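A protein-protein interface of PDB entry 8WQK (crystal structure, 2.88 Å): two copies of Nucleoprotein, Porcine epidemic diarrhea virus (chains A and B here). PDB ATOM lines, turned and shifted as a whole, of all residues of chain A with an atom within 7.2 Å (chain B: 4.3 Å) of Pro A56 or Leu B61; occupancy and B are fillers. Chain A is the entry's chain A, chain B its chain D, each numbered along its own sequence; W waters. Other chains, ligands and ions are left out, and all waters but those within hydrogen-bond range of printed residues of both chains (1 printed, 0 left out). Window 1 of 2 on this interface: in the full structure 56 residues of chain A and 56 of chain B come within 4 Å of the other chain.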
ATOM      1  N   GLU A   9       1.808  32.302 -12.420  1.00  0.00           N
ATOM      2  CA  GLU A   9       0.381  32.071 -12.231  1.00  0.00           C
ATOM      3  C   GLU A   9      -0.064  30.737 -12.801  1.00  0.00           C
ATOM      4  O   GLU A   9      -0.855  30.026 -12.170  1.00  0.00           O
ATOM      5  CB  GLU A   9      -0.415  33.210 -12.869  1.00  0.00           C
ATOM      6  CG  GLU A   9      -0.940  34.222 -11.869  1.00  0.00           C
ATOM      7  CD  GLU A   9      -2.133  34.998 -12.396  1.00  0.00           C
ATOM      8  OE1 GLU A   9      -3.099  34.354 -12.864  1.00  0.00           O
ATOM      9  OE2 GLU A   9      -2.112  36.250 -12.324  1.00  0.00           O
ATOM     10  N   TRP A  10       0.469  30.351 -13.967  1.00  0.00           N
ATOM     11  CA  TRP A  10      -0.051  29.142 -14.615  1.00  0.00           C
ATOM     12  C   TRP A  10       0.363  27.859 -13.907  1.00  0.00           C
ATOM     13  O   TRP A  10      -0.143  26.782 -14.260  1.00  0.00           O
ATOM     14  CB  TRP A  10       0.372  29.090 -16.088  1.00  0.00           C
ATOM     15  CG  TRP A  10       1.850  29.053 -16.317  1.00  0.00           C
ATOM     16  CD1 TRP A  10       2.634  27.937 -16.454  1.00  0.00           C
ATOM     17  CD2 TRP A  10       2.733  30.190 -16.448  1.00  0.00           C
ATOM     18  NE1 TRP A  10       3.951  28.313 -16.652  1.00  0.00           N
ATOM     19  CE2 TRP A  10       4.034  29.686 -16.652  1.00  0.00           C
ATOM     20  CE3 TRP A  10       2.546  31.581 -16.414  1.00  0.00           C
ATOM     21  CZ2 TRP A  10       5.134  30.521 -16.825  1.00  0.00           C
ATOM     22  CZ3 TRP A  10       3.653  32.415 -16.581  1.00  0.00           C
ATOM     23  CH2 TRP A  10       4.920  31.881 -16.786  1.00  0.00           C
ATOM     24  N   ARG A  12       0.228  27.811 -10.285  1.00  0.00           N
ATOM     25  CA  ARG A  12      -0.291  27.881  -8.934  1.00  0.00           C
ATOM     26  C   ARG A  12      -1.399  26.856  -8.717  1.00  0.00           C
ATOM     27  O   ARG A  12      -2.076  26.436  -9.660  1.00  0.00           O
ATOM     28  CB  ARG A  12      -0.807  29.280  -8.668  1.00  0.00           C
ATOM     29  CG  ARG A  12       0.290  30.217  -8.324  1.00  0.00           C
ATOM     30  CD  ARG A  12      -0.072  31.661  -8.582  1.00  0.00           C
ATOM     31  NE  ARG A  12       1.141  32.469  -8.549  1.00  0.00           N
ATOM     32  CZ  ARG A  12       1.182  33.772  -8.313  1.00  0.00           C
ATOM     33  NH1 ARG A  12       0.082  34.467  -8.069  1.00  0.00           N
ATOM     34  NH2 ARG A  12       2.359  34.389  -8.313  1.00  0.00           N
ATOM     35  N   PHE A  24      -5.018  34.113  -7.963  1.00  0.00           N
ATOM     36  CA  PHE A  24      -5.550  34.619  -9.214  1.00  0.00           C
ATOM     37  C   PHE A  24      -6.275  35.952  -9.097  1.00  0.00           C
ATOM     38  O   PHE A  24      -6.714  36.489 -10.119  1.00  0.00           O
ATOM     39  CB  PHE A  24      -6.468  33.556  -9.838  1.00  0.00           C
ATOM     40  CG  PHE A  24      -5.830  32.195  -9.889  1.00  0.00           C
ATOM     41  CD1 PHE A  24      -4.779  31.950 -10.747  1.00  0.00           C
ATOM     42  CD2 PHE A  24      -6.230  31.187  -9.027  1.00  0.00           C
ATOM     43  CE1 PHE A  24      -4.161  30.713 -10.770  1.00  0.00           C
ATOM     44  CE2 PHE A  24      -5.616  29.947  -9.044  1.00  0.00           C
ATOM     45  CZ  PHE A  24      -4.577  29.714  -9.912  1.00  0.00           C
ATOM     46  N   ARG A  27     -12.613  37.488  -8.663  1.00  0.00           N
ATOM     47  CA  ARG A  27     -13.426  37.017  -9.772  1.00  0.00           C
ATOM     48  C   ARG A  27     -13.879  38.211 -10.585  1.00  0.00           C
ATOM     49  O   ARG A  27     -14.176  39.277 -10.043  1.00  0.00           O
ATOM     50  CB  ARG A  27     -14.678  36.273  -9.291  1.00  0.00           C
ATOM     51  CG  ARG A  27     -14.481  35.014  -8.460  1.00  0.00           C
ATOM     52  CD  ARG A  27     -13.045  34.519  -8.474  1.00  0.00           C
ATOM     53  NE  ARG A  27     -12.761  33.694  -9.635  1.00  0.00           N
ATOM     54  CZ  ARG A  27     -11.541  33.421 -10.068  1.00  0.00           C
ATOM     55  NH1 ARG A  27     -10.472  33.927  -9.479  1.00  0.00           N
ATOM     56  NH2 ARG A  27     -11.393  32.626 -11.127  1.00  0.00           N
ATOM     57  N   PHE A  33     -14.946  32.034 -12.988  1.00  0.00           N
ATOM     58  CA  PHE A  33     -15.380  30.743 -12.477  1.00  0.00           C
ATOM     59  C   PHE A  33     -15.219  30.690 -10.970  1.00  0.00           C
ATOM     60  O   PHE A  33     -14.175  31.073 -10.438  1.00  0.00           O
ATOM     61  CB  PHE A  33     -14.570  29.622 -13.123  1.00  0.00           C
ATOM     62  CG  PHE A  33     -14.933  28.249 -12.648  1.00  0.00           C
ATOM     63  CD1 PHE A  33     -14.336  27.706 -11.521  1.00  0.00           C
ATOM     64  CD2 PHE A  33     -15.867  27.495 -13.341  1.00  0.00           C
ATOM     65  CE1 PHE A  33     -14.670  26.427 -11.089  1.00  0.00           C
ATOM     66  CE2 PHE A  33     -16.205  26.211 -12.923  1.00  0.00           C
ATOM     67  CZ  PHE A  33     -15.610  25.680 -11.792  1.00  0.00           C
ATOM     68  N   TYR A  48     -14.890  20.010  -6.495  1.00  0.00           N
ATOM     69  CA  TYR A  48     -13.791  20.366  -7.394  1.00  0.00           C
ATOM     70  C   TYR A  48     -13.295  19.168  -8.184  1.00  0.00           C
ATOM     71  O   TYR A  48     -13.100  19.251  -9.403  1.00  0.00           O
ATOM     72  CB  TYR A  48     -12.628  20.969  -6.619  1.00  0.00           C
ATOM     73  CG  TYR A  48     -11.406  21.191  -7.476  1.00  0.00           C
ATOM     74  CD1 TYR A  48     -10.434  20.201  -7.619  1.00  0.00           C
ATOM     75  CD2 TYR A  48     -11.217  22.397  -8.131  1.00  0.00           C
ATOM     76  CE1 TYR A  48      -9.312  20.401  -8.408  1.00  0.00           C
ATOM     77  CE2 TYR A  48     -10.095  22.614  -8.917  1.00  0.00           C
ATOM     78  CZ  TYR A  48      -9.144  21.610  -9.056  1.00  0.00           C
ATOM     79  OH  TYR A  48      -8.026  21.835  -9.835  1.00  0.00           O
ATOM     80  N   ALA A  52     -12.852  19.166 -12.050  1.00  0.00           N
ATOM     81  CA  ALA A  52     -11.539  19.092 -12.688  1.00  0.00           C
ATOM     82  C   ALA A  52     -11.459  17.993 -13.738  1.00  0.00           C
ATOM     83  O   ALA A  52     -10.628  18.086 -14.645  1.00  0.00           O
ATOM     84  CB  ALA A  52     -10.446  18.883 -11.644  1.00  0.00           C
ATOM     85  N   SER A  53     -12.331  16.984 -13.671  1.00  0.00           N
ATOM     86  CA  SER A  53     -12.370  15.945 -14.696  1.00  0.00           C
ATOM     87  C   SER A  53     -12.908  16.452 -16.025  1.00  0.00           C
ATOM     88  O   SER A  53     -12.849  15.725 -17.023  1.00  0.00           O
ATOM     89  CB  SER A  53     -13.227  14.763 -14.226  1.00  0.00           C
ATOM     90  OG  SER A  53     -14.603  15.103 -14.248  1.00  0.00           O
ATOM     91  N   LEU A  54     -13.463  17.657 -16.059  1.00  0.00           N
ATOM     92  CA  LEU A  54     -13.960  18.251 -17.287  1.00  0.00           C
ATOM     93  C   LEU A  54     -13.074  19.418 -17.725  1.00  0.00           C
ATOM     94  O   LEU A  54     -13.545  20.392 -18.314  1.00  0.00           O
ATOM     95  CB  LEU A  54     -15.410  18.686 -17.092  1.00  0.00           C
ATOM     96  CG  LEU A  54     -16.358  17.567 -16.633  1.00  0.00           C
ATOM     97  CD1 LEU A  54     -17.738  18.098 -16.364  1.00  0.00           C
ATOM     98  CD2 LEU A  54     -16.417  16.456 -17.685  1.00  0.00           C
ATOM     99  N   ALA A  55     -11.774  19.305 -17.481  1.00  0.00           N
ATOM    100  CA  ALA A  55     -10.842  20.310 -17.904  1.00  0.00           C
ATOM    101  C   ALA A  55      -9.626  19.569 -18.440  1.00  0.00           C
ATOM    102  O   ALA A  55      -9.265  18.500 -17.919  1.00  0.00           O
ATOM    103  CB  ALA A  55     -10.429  21.260 -16.781  1.00  0.00           C
ATOM    104  N   PRO A  56      -9.031  20.076 -19.513  1.00  0.00           N
ATOM    105  CA  PRO A  56      -7.992  19.327 -20.226  1.00  0.00           C
ATOM    106  C   PRO A  56      -6.632  19.335 -19.542  1.00  0.00           C
ATOM    107  O   PRO A  56      -6.186  20.352 -19.004  1.00  0.00           O
ATOM    108  CB  PRO A  56      -7.920  20.061 -21.568  1.00  0.00           C
ATOM    109  CG  PRO A  56      -8.328  21.477 -21.219  1.00  0.00           C
ATOM    110  CD  PRO A  56      -9.441  21.295 -20.231  1.00  0.00           C
ATOM    111  N   ASN A  57      -5.921  18.206 -19.660  1.00  0.00           N
ATOM    112  CA  ASN A  57      -4.530  18.161 -19.213  1.00  0.00           C
ATOM    113  C   ASN A  57      -3.641  18.917 -20.193  1.00  0.00           C
ATOM    114  O   ASN A  57      -4.083  19.379 -21.251  1.00  0.00           O
ATOM    115  CB  ASN A  57      -4.036  16.732 -19.048  1.00  0.00           C
ATOM    116  CG  ASN A  57      -4.032  15.960 -20.348  1.00  0.00           C
ATOM    117  OD1 ASN A  57      -3.662  16.471 -21.401  1.00  0.00           O
ATOM    118  ND2 ASN A  57      -4.422  14.699 -20.273  1.00  0.00           N
ATOM    119  N   VAL A  58      -2.356  19.024 -19.852  1.00  0.00           N
ATOM    120  CA  VAL A  58      -1.473  19.864 -20.654  1.00  0.00           C
ATOM    121  C   VAL A  58      -1.350  19.325 -22.073  1.00  0.00           C
ATOM    122  O   VAL A  58      -1.470  20.083 -23.041  1.00  0.00           O
ATOM    123  CB  VAL A  58      -0.102  19.990 -19.983  1.00  0.00           C
ATOM    124  CG1 VAL A  58       0.888  20.509 -20.980  1.00  0.00           C
ATOM    125  CG2 VAL A  58      -0.185  20.890 -18.801  1.00  0.00           C
ATOM    126  N   ALA A  59      -1.180  18.009 -22.234  1.00  0.00           N
ATOM    127  CA  ALA A  59      -1.020  17.473 -23.587  1.00  0.00           C
ATOM    128  C   ALA A  59      -2.244  17.762 -24.452  1.00  0.00           C
ATOM    129  O   ALA A  59      -2.107  18.033 -25.648  1.00  0.00           O
ATOM    130  CB  ALA A  59      -0.721  15.980 -23.544  1.00  0.00           C
ATOM    131  N   ALA A  60      -3.453  17.690 -23.876  1.00  0.00           N
ATOM    132  CA  ALA A  60      -4.660  18.078 -24.610  1.00  0.00           C
ATOM    133  C   ALA A  60      -4.734  19.590 -24.839  1.00  0.00           C
ATOM    134  O   ALA A  60      -5.285  20.033 -25.852  1.00  0.00           O
ATOM    135  CB  ALA A  60      -5.909  17.591 -23.888  1.00  0.00           C
ATOM    136  N   LEU A  61      -4.214  20.400 -23.912  1.00  0.00           N
ATOM    137  CA  LEU A  61      -4.212  21.847 -24.115  1.00  0.00           C
ATOM    138  C   LEU A  61      -3.391  22.242 -25.337  1.00  0.00           C
ATOM    139  O   LEU A  61      -3.811  23.101 -26.122  1.00  0.00           O
ATOM    140  CB  LEU A  61      -3.639  22.553 -22.885  1.00  0.00           C
ATOM    141  CG  LEU A  61      -4.547  23.101 -21.793  1.00  0.00           C
ATOM    142  CD1 LEU A  61      -3.700  23.855 -20.800  1.00  0.00           C
ATOM    143  CD2 LEU A  61      -5.643  23.984 -22.397  1.00  0.00           C
ATOM    144  N   LEU A  62      -2.223  21.617 -25.520  1.00  0.00           N
ATOM    145  CA  LEU A  62      -1.323  21.974 -26.613  1.00  0.00           C
ATOM    146  C   LEU A  62      -1.765  21.340 -27.923  1.00  0.00           C
ATOM    147  O   LEU A  62      -1.760  21.993 -28.972  1.00  0.00           O
ATOM    148  CB  LEU A  62       0.102  21.542 -26.294  1.00  0.00           C
ATOM    149  CG  LEU A  62       0.779  22.042 -25.029  1.00  0.00           C
ATOM    150  CD1 LEU A  62       1.838  21.041 -24.592  1.00  0.00           C
ATOM    151  CD2 LEU A  62       1.413  23.397 -25.324  1.00  0.00           C
ATOM    152  N   TYR A  80      -4.227  30.216 -24.636  1.00  0.00           N
ATOM    153  CA  TYR A  80      -4.789  28.919 -24.952  1.00  0.00           C
ATOM    154  C   TYR A  80      -6.300  29.057 -25.049  1.00  0.00           C
ATOM    155  O   TYR A  80      -6.920  29.690 -24.192  1.00  0.00           O
ATOM    156  CB  TYR A  80      -4.434  27.899 -23.884  1.00  0.00           C
ATOM    157  CG  TYR A  80      -2.960  27.639 -23.701  1.00  0.00           C
ATOM    158  CD1 TYR A  80      -2.314  26.653 -24.423  1.00  0.00           C
ATOM    159  CD2 TYR A  80      -2.223  28.351 -22.775  1.00  0.00           C
ATOM    160  CE1 TYR A  80      -0.976  26.396 -24.231  1.00  0.00           C
ATOM    161  CE2 TYR A  80      -0.887  28.094 -22.575  1.00  0.00           C
ATOM    162  CZ  TYR A  80      -0.277  27.120 -23.303  1.00  0.00           C
ATOM    163  OH  TYR A  80       1.049  26.867 -23.095  1.00  0.00           O
ATOM    164  N   TYR A  82      -9.296  26.350 -25.699  1.00  0.00           N
ATOM    165  CA  TYR A  82      -9.599  24.924 -25.793  1.00  0.00           C
ATOM    166  C   TYR A  82     -11.101  24.730 -25.635  1.00  0.00           C
ATOM    167  O   TYR A  82     -11.652  24.959 -24.552  1.00  0.00           O
ATOM    168  CB  TYR A  82      -8.843  24.125 -24.735  1.00  0.00           C
ATOM    169  CG  TYR A  82      -9.033  22.635 -24.880  1.00  0.00           C
ATOM    170  CD1 TYR A  82     -10.136  21.986 -24.339  1.00  0.00           C
ATOM    171  CD2 TYR A  82      -8.110  21.877 -25.572  1.00  0.00           C
ATOM    172  CE1 TYR A  82     -10.299  20.630 -24.479  1.00  0.00           C
ATOM    173  CE2 TYR A  82      -8.267  20.523 -25.709  1.00  0.00           C
ATOM    174  CZ  TYR A  82      -9.359  19.905 -25.167  1.00  0.00           C
ATOM    175  OH  TYR A  82      -9.489  18.545 -25.354  1.00  0.00           O
ATOM    176  N   LYS A  83     -11.752  24.285 -26.699  1.00  0.00           N
ATOM    177  CA  LYS A  83     -13.169  23.972 -26.690  1.00  0.00           C
ATOM    178  C   LYS A  83     -13.387  22.469 -26.534  1.00  0.00           C
ATOM    179  O   LYS A  83     -12.564  21.663 -26.973  1.00  0.00           O
ATOM    180  CB  LYS A  83     -13.802  24.489 -27.974  1.00  0.00           C
ATOM    181  CG  LYS A  83     -13.499  25.963 -28.217  1.00  0.00           C
ATOM    182  CD  LYS A  83     -14.266  26.483 -29.423  1.00  0.00           C
ATOM    183  CE  LYS A  83     -15.781  26.464 -29.174  1.00  0.00           C
ATOM    184  NZ  LYS A  83     -16.382  25.173 -29.641  1.00  0.00           N
ATOM    185  N   MET A  84     -14.497  22.100 -25.886  1.00  0.00           N
ATOM    186  CA  MET A  84     -14.869  20.700 -25.724  1.00  0.00           C
ATOM    187  C   MET A  84     -16.372  20.581 -25.472  1.00  0.00           C
ATOM    188  O   MET A  84     -17.015  21.523 -25.001  1.00  0.00           O
ATOM    189  CB  MET A  84     -14.080  20.064 -24.578  1.00  0.00           C
ATOM    190  CG  MET A  84     -14.227  20.829 -23.282  1.00  0.00           C
ATOM    191  SD  MET A  84     -13.272  20.110 -21.940  1.00  0.00           S
ATOM    192  CE  MET A  84     -14.483  19.062 -21.133  1.00  0.00           C
ATOM    193  N   TRP B  10     -10.232  15.404 -23.895  1.00  0.00           N
ATOM    194  CA  TRP B  10      -9.535  16.409 -23.104  1.00  0.00           C
ATOM    195  C   TRP B  10      -8.661  15.832 -22.005  1.00  0.00           C
ATOM    196  O   TRP B  10      -7.986  16.609 -21.323  1.00  0.00           O
ATOM    197  CB  TRP B  10     -10.529  17.363 -22.461  1.00  0.00           C
ATOM    198  CG  TRP B  10     -11.546  16.694 -21.575  1.00  0.00           C
ATOM    199  CD1 TRP B  10     -11.400  16.422 -20.251  1.00  0.00           C
ATOM    200  CD2 TRP B  10     -12.868  16.254 -21.930  1.00  0.00           C
ATOM    201  NE1 TRP B  10     -12.527  15.831 -19.761  1.00  0.00           N
ATOM    202  CE2 TRP B  10     -13.451  15.718 -20.768  1.00  0.00           C
ATOM    203  CE3 TRP B  10     -13.614  16.254 -23.117  1.00  0.00           C
ATOM    204  CZ2 TRP B  10     -14.750  15.187 -20.751  1.00  0.00           C
ATOM    205  CZ3 TRP B  10     -14.907  15.730 -23.095  1.00  0.00           C
ATOM    206  CH2 TRP B  10     -15.457  15.202 -21.921  1.00  0.00           C
ATOM    207  N   PRO B  56      -0.813  25.782 -18.437  1.00  0.00           N
ATOM    208  CA  PRO B  56      -1.441  25.772 -17.107  1.00  0.00           C
ATOM    209  C   PRO B  56      -2.031  24.438 -16.680  1.00  0.00           C
ATOM    210  O   PRO B  56      -2.545  23.665 -17.488  1.00  0.00           O
ATOM    211  CB  PRO B  56      -2.555  26.808 -17.254  1.00  0.00           C
ATOM    212  CG  PRO B  56      -2.934  26.688 -18.685  1.00  0.00           C
ATOM    213  CD  PRO B  56      -1.658  26.471 -19.425  1.00  0.00           C
ATOM    214  N   ASN B  57      -1.989  24.196 -15.369  1.00  0.00           N
ATOM    215  CA  ASN B  57      -2.698  23.081 -14.756  1.00  0.00           C
ATOM    216  C   ASN B  57      -4.200  23.383 -14.658  1.00  0.00           C
ATOM    217  O   ASN B  57      -4.653  24.512 -14.874  1.00  0.00           O
ATOM    218  CB  ASN B  57      -2.126  22.800 -13.373  1.00  0.00           C
ATOM    219  CG  ASN B  57      -2.253  23.997 -12.456  1.00  0.00           C
ATOM    220  OD1 ASN B  57      -3.358  24.362 -12.055  1.00  0.00           O
ATOM    221  ND2 ASN B  57      -1.127  24.638 -12.141  1.00  0.00           N
ATOM    222  N   VAL B  58      -4.974  22.365 -14.258  1.00  0.00           N
ATOM    223  CA  VAL B  58      -6.432  22.477 -14.282  1.00  0.00           C
ATOM    224  C   VAL B  58      -6.915  23.537 -13.307  1.00  0.00           C
ATOM    225  O   VAL B  58      -7.831  24.312 -13.615  1.00  0.00           O
ATOM    226  CB  VAL B  58      -7.082  21.117 -13.981  1.00  0.00           C
ATOM    227  CG1 VAL B  58      -8.581  21.299 -13.781  1.00  0.00           C
ATOM    228  CG2 VAL B  58      -6.791  20.159 -15.092  1.00  0.00           C
ATOM    229  N   ALA B  59      -6.337  23.573 -12.106  1.00  0.00           N
ATOM    230  CA  ALA B  59      -6.772  24.572 -11.132  1.00  0.00           C
ATOM    231  C   ALA B  59      -6.521  25.978 -11.659  1.00  0.00           C
ATOM    232  O   ALA B  59      -7.368  26.871 -11.504  1.00  0.00           O
ATOM    233  CB  ALA B  59      -6.068  24.361  -9.792  1.00  0.00           C
ATOM    234  N   ALA B  60      -5.375  26.177 -12.321  1.00  0.00           N
ATOM    235  CA  ALA B  60      -5.070  27.456 -12.949  1.00  0.00           C
ATOM    236  C   ALA B  60      -5.974  27.719 -14.140  1.00  0.00           C
ATOM    237  O   ALA B  60      -6.293  28.874 -14.444  1.00  0.00           O
ATOM    238  CB  ALA B  60      -3.613  27.472 -13.397  1.00  0.00           C
ATOM    239  N   LEU B  61      -6.340  26.672 -14.862  1.00  0.00           N
ATOM    240  CA  LEU B  61      -7.232  26.827 -15.998  1.00  0.00           C
ATOM    241  C   LEU B  61      -8.629  27.272 -15.568  1.00  0.00           C
ATOM    242  O   LEU B  61      -9.236  28.141 -16.210  1.00  0.00           O
ATOM    243  CB  LEU B  61      -7.276  25.507 -16.759  1.00  0.00           C
ATOM    244  CG  LEU B  61      -7.589  25.522 -18.238  1.00  0.00           C
ATOM    245  CD1 LEU B  61      -6.499  26.213 -19.025  1.00  0.00           C
ATOM    246  CD2 LEU B  61      -7.749  24.079 -18.675  1.00  0.00           C
ATOM    247  N   LEU B  62      -9.139  26.706 -14.464  1.00  0.00           N
ATOM    248  CA  LEU B  62     -10.496  26.982 -14.005  1.00  0.00           C
ATOM    249  C   LEU B  62     -10.563  28.324 -13.288  1.00  0.00           C
ATOM    250  O   LEU B  62     -11.532  29.069 -13.465  1.00  0.00           O
ATOM    251  CB  LEU B  62     -11.004  25.854 -13.084  1.00  0.00           C
ATOM    252  CG  LEU B  62     -11.351  24.438 -13.603  1.00  0.00           C
ATOM    253  CD1 LEU B  62     -11.304  23.478 -12.452  1.00  0.00           C
ATOM    254  CD2 LEU B  62     -12.716  24.297 -14.310  1.00  0.00           C
ATOM    255  N   PHE B  63      -9.568  28.622 -12.437  1.00  0.00           N
ATOM    256  CA  PHE B  63      -9.549  29.822 -11.612  1.00  0.00           C
ATOM    257  C   PHE B  63      -8.730  30.970 -12.190  1.00  0.00           C
ATOM    258  O   PHE B  63      -8.915  32.112 -11.760  1.00  0.00           O
ATOM    259  CB  PHE B  63      -8.979  29.502 -10.232  1.00  0.00           C
ATOM    260  CG  PHE B  63      -9.820  28.560  -9.425  1.00  0.00           C
ATOM    261  CD1 PHE B  63     -11.106  28.897  -9.062  1.00  0.00           C
ATOM    262  CD2 PHE B  63      -9.314  27.345  -9.017  1.00  0.00           C
ATOM    263  CE1 PHE B  63     -11.868  28.035  -8.324  1.00  0.00           C
ATOM    264  CE2 PHE B  63     -10.064  26.488  -8.267  1.00  0.00           C
ATOM    265  CZ  PHE B  63     -11.345  26.830  -7.922  1.00  0.00           C
ATOM    266  N   GLY B  64      -7.822  30.715 -13.129  1.00  0.00           N
ATOM    267  CA  GLY B  64      -6.955  31.767 -13.611  1.00  0.00           C
ATOM    268  C   GLY B  64      -7.209  32.199 -15.038  1.00  0.00           C
ATOM    269  O   GLY B  64      -6.500  33.070 -15.555  1.00  0.00           O
ATOM    270  N   GLY B  65      -8.234  31.635 -15.669  1.00  0.00           N
ATOM    271  CA  GLY B  65      -8.620  31.994 -17.019  1.00  0.00           C
ATOM    272  C   GLY B  65     -10.120  32.157 -17.144  1.00  0.00           C
ATOM    273  O   GLY B  65     -10.802  32.330 -16.128  1.00  0.00           O
ATOM    274  N   TYR B  80     -12.406  27.012 -22.578  1.00  0.00           N
ATOM    275  CA  TYR B  80     -11.411  27.592 -21.680  1.00  0.00           C
ATOM    276  C   TYR B  80     -10.569  28.591 -22.457  1.00  0.00           C
ATOM    277  O   TYR B  80     -10.177  28.319 -23.590  1.00  0.00           O
ATOM    278  CB  TYR B  80     -10.512  26.510 -21.080  1.00  0.00           C
ATOM    279  CG  TYR B  80     -11.249  25.539 -20.212  1.00  0.00           C
ATOM    280  CD1 TYR B  80     -11.422  25.789 -18.855  1.00  0.00           C
ATOM    281  CD2 TYR B  80     -11.789  24.383 -20.743  1.00  0.00           C
ATOM    282  CE1 TYR B  80     -12.102  24.925 -18.055  1.00  0.00           C
ATOM    283  CE2 TYR B  80     -12.478  23.498 -19.943  1.00  0.00           C
ATOM    284  CZ  TYR B  80     -12.636  23.778 -18.596  1.00  0.00           C
ATOM    285  OH  TYR B  80     -13.316  22.892 -17.783  1.00  0.00           O
ATOM    286  N   TYR B  82      -7.255  30.850 -21.574  1.00  0.00           N
ATOM    287  CA  TYR B  82      -6.242  31.111 -20.555  1.00  0.00           C
ATOM    288  C   TYR B  82      -5.119  31.971 -21.144  1.00  0.00           C
ATOM    289  O   TYR B  82      -4.390  31.531 -22.037  1.00  0.00           O
ATOM    290  CB  TYR B  82      -5.713  29.806 -19.964  1.00  0.00           C
ATOM    291  CG  TYR B  82      -4.824  30.109 -18.803  1.00  0.00           C
ATOM    292  CD1 TYR B  82      -5.357  30.440 -17.552  1.00  0.00           C
ATOM    293  CD2 TYR B  82      -3.448  30.154 -18.963  1.00  0.00           C
ATOM    294  CE1 TYR B  82      -4.521  30.762 -16.468  1.00  0.00           C
ATOM    295  CE2 TYR B  82      -2.604  30.475 -17.896  1.00  0.00           C
ATOM    296  CZ  TYR B  82      -3.137  30.787 -16.661  1.00  0.00           C
ATOM    297  OH  TYR B  82      -2.272  31.121 -15.636  1.00  0.00           O
HETATM  298  O   HOH W   1      -3.803  20.681 -17.425  1.00  0.00           O
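The guanidinium group (NE) of Arg A27 lies within hydrogen-bond range of the backbone carbonyl oxygen (O) of Phe A33, at 3.1 Å.
OD1 of Asn A57 lies within hydrogen-bond range of N of Ala A59.
The side-chain amide oxygen of Asn A57 is in hydrogen-bond range of the backbone NH of Ala A60 (2.8 Å).
OD1 of Asn B57 is in hydrogen-bond range of N of Ala B59.
The side-chain amide oxygen (OD1) of Asn B57 is in hydrogen-bond range of the backbone NH (N) of Ala B60 (2.7 Å).
Of the 22 printed residues of chain A, 19 touch a printed residue of chain B.
Hydrophobic or aromatic side chains of chain A within 4 Å of the printed part of chain B: Trp A10, Phe A24, Phe A33, Tyr A48, Ala A52, Leu A54, Ala A55, Pro A56, Val A58, Ala A60, Leu A61, Tyr A80, Tyr A82 and Met A84.
Along chain A the printed residues that touch a printed residue of chain B span positions 9 to 84.
Of the 13 printed residues of chain B, 12 touch a printed residue of chain A.
Hydrophobic or aromatic side chains of chain B that line the printed part of chain A: Trp B10, Pro B56, Val B58, Ala B59, Ala B60, Leu B61, Leu B62, Phe B63, Tyr B80 and Tyr B82.
Along chain B the printed residues that touch a printed residue of chain A span positions 10 to 82.
Among the printed residues, 36 pairs touch across the chains.
Trp A10 touches Ala B60 (O to CB, 3.6 Å).
CB of Phe A24 touches O of Phe B63 (3.4 Å).
Gly B64 touches Phe A24.
CB of Phe A33 touches O of Leu B62, 3.1 Å away.
Phe B63 touches Tyr A48 (CE2 to CE2, 3.9 Å).
Ala A52 touches Val B58.
CD2 of Leu A54 touches CZ2 of Trp B10, at 3.7 Å.
Ala A55 touches Tyr B80 (CB to OH, 3.5 Å).
Pro A56 touches Val B58.
Pro B56 touches Leu A61.
Water W1 lies within hydrogen-bond range of O of Pro A56, O of Pro B56 and N of Val A58.
The backbone carbonyl oxygen (O) of Trp A10 lies within hydrogen-bond range of the side-chain amide nitrogen (ND2) of Asn B57, 3.2 Å away.
The backbone NH (N) of Trp A10 lies close to the side-chain hydroxyl (OH) of Tyr B82, at 3.3 Å.
The side-chain amide nitrogen of Asn B57 lies within hydrogen-bond range of the backbone carbonyl oxygen of Arg A12 (3.2 Å).
The backbone carbonyl oxygen of Phe B63 lies within hydrogen-bond range of the guanidinium group of Arg A27 (2.6 Å).
OH of Tyr A48 sits close to N of Ala B59, at 3.3 Å.
The indole nitrogen (NE1) of Trp B10 is in hydrogen-bond range of the backbone carbonyl oxygen (O) of Ser A53 (2.8 Å).
The side-chain hydroxyl (OH) of Tyr B80 lies within hydrogen-bond range of the backbone carbonyl oxygen (O) of Leu A54 (2.6 Å).
The backbone NH (N) of Asn A57 is in hydrogen-bond range of the backbone carbonyl oxygen (O) of Trp B10.
The backbone carbonyl oxygen (O) of Tyr A80 is in hydrogen-bond range of the backbone NH (N) of Tyr B82, 2.9 Å away.
The backbone carbonyl oxygen (O) of Tyr A82 sits at hydrogen-bond distance from the backbone NH (N) of Tyr B80 (2.9 Å).
Printed residues of chain B within 4 Å of Phe A33: Leu B62 (3.1 Å).
Pro A56 touches just these residues of chain B: Trp B10 (2.9 Å), Val B58 (3.96 Å), Leu B61 (3.6 Å) and Tyr B80 (3.8 Å).
Lys A83 touches none of the printed residues of chain B.
Of the printed residues of chain A, Trp B10 touches Ser A53 (2.8 Å), Leu A54 (3.7 Å), Ala A55 (3.8 Å), Pro A56 (2.9 Å), Asn A57 (3.1 Å), Ala A60 (3.4 Å), Tyr A82 (3.1 Å) and Met A84 (3.3 Å).
Of chain A, only Pro A56 comes within 4 Å of Leu B61.
The nearest residue of chain A that does not touch Leu B61 is Leu A61 (4.1 Å).
Pro A56 touches Leu B61, and with the chains exchanged Leu A61 touches Pro B56.
Pro A56 touches Tyr B80, and with the chains exchanged Tyr A80 touches Pro B56.
Tyr A80 touches Tyr B82, and with the chains exchanged Tyr A82 touches Tyr B80.
10 positions are printed for both chains.
Of the 36 pairs that touch across the chains among the printed residues, 17 have their exchanged pair printed and touching as well.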
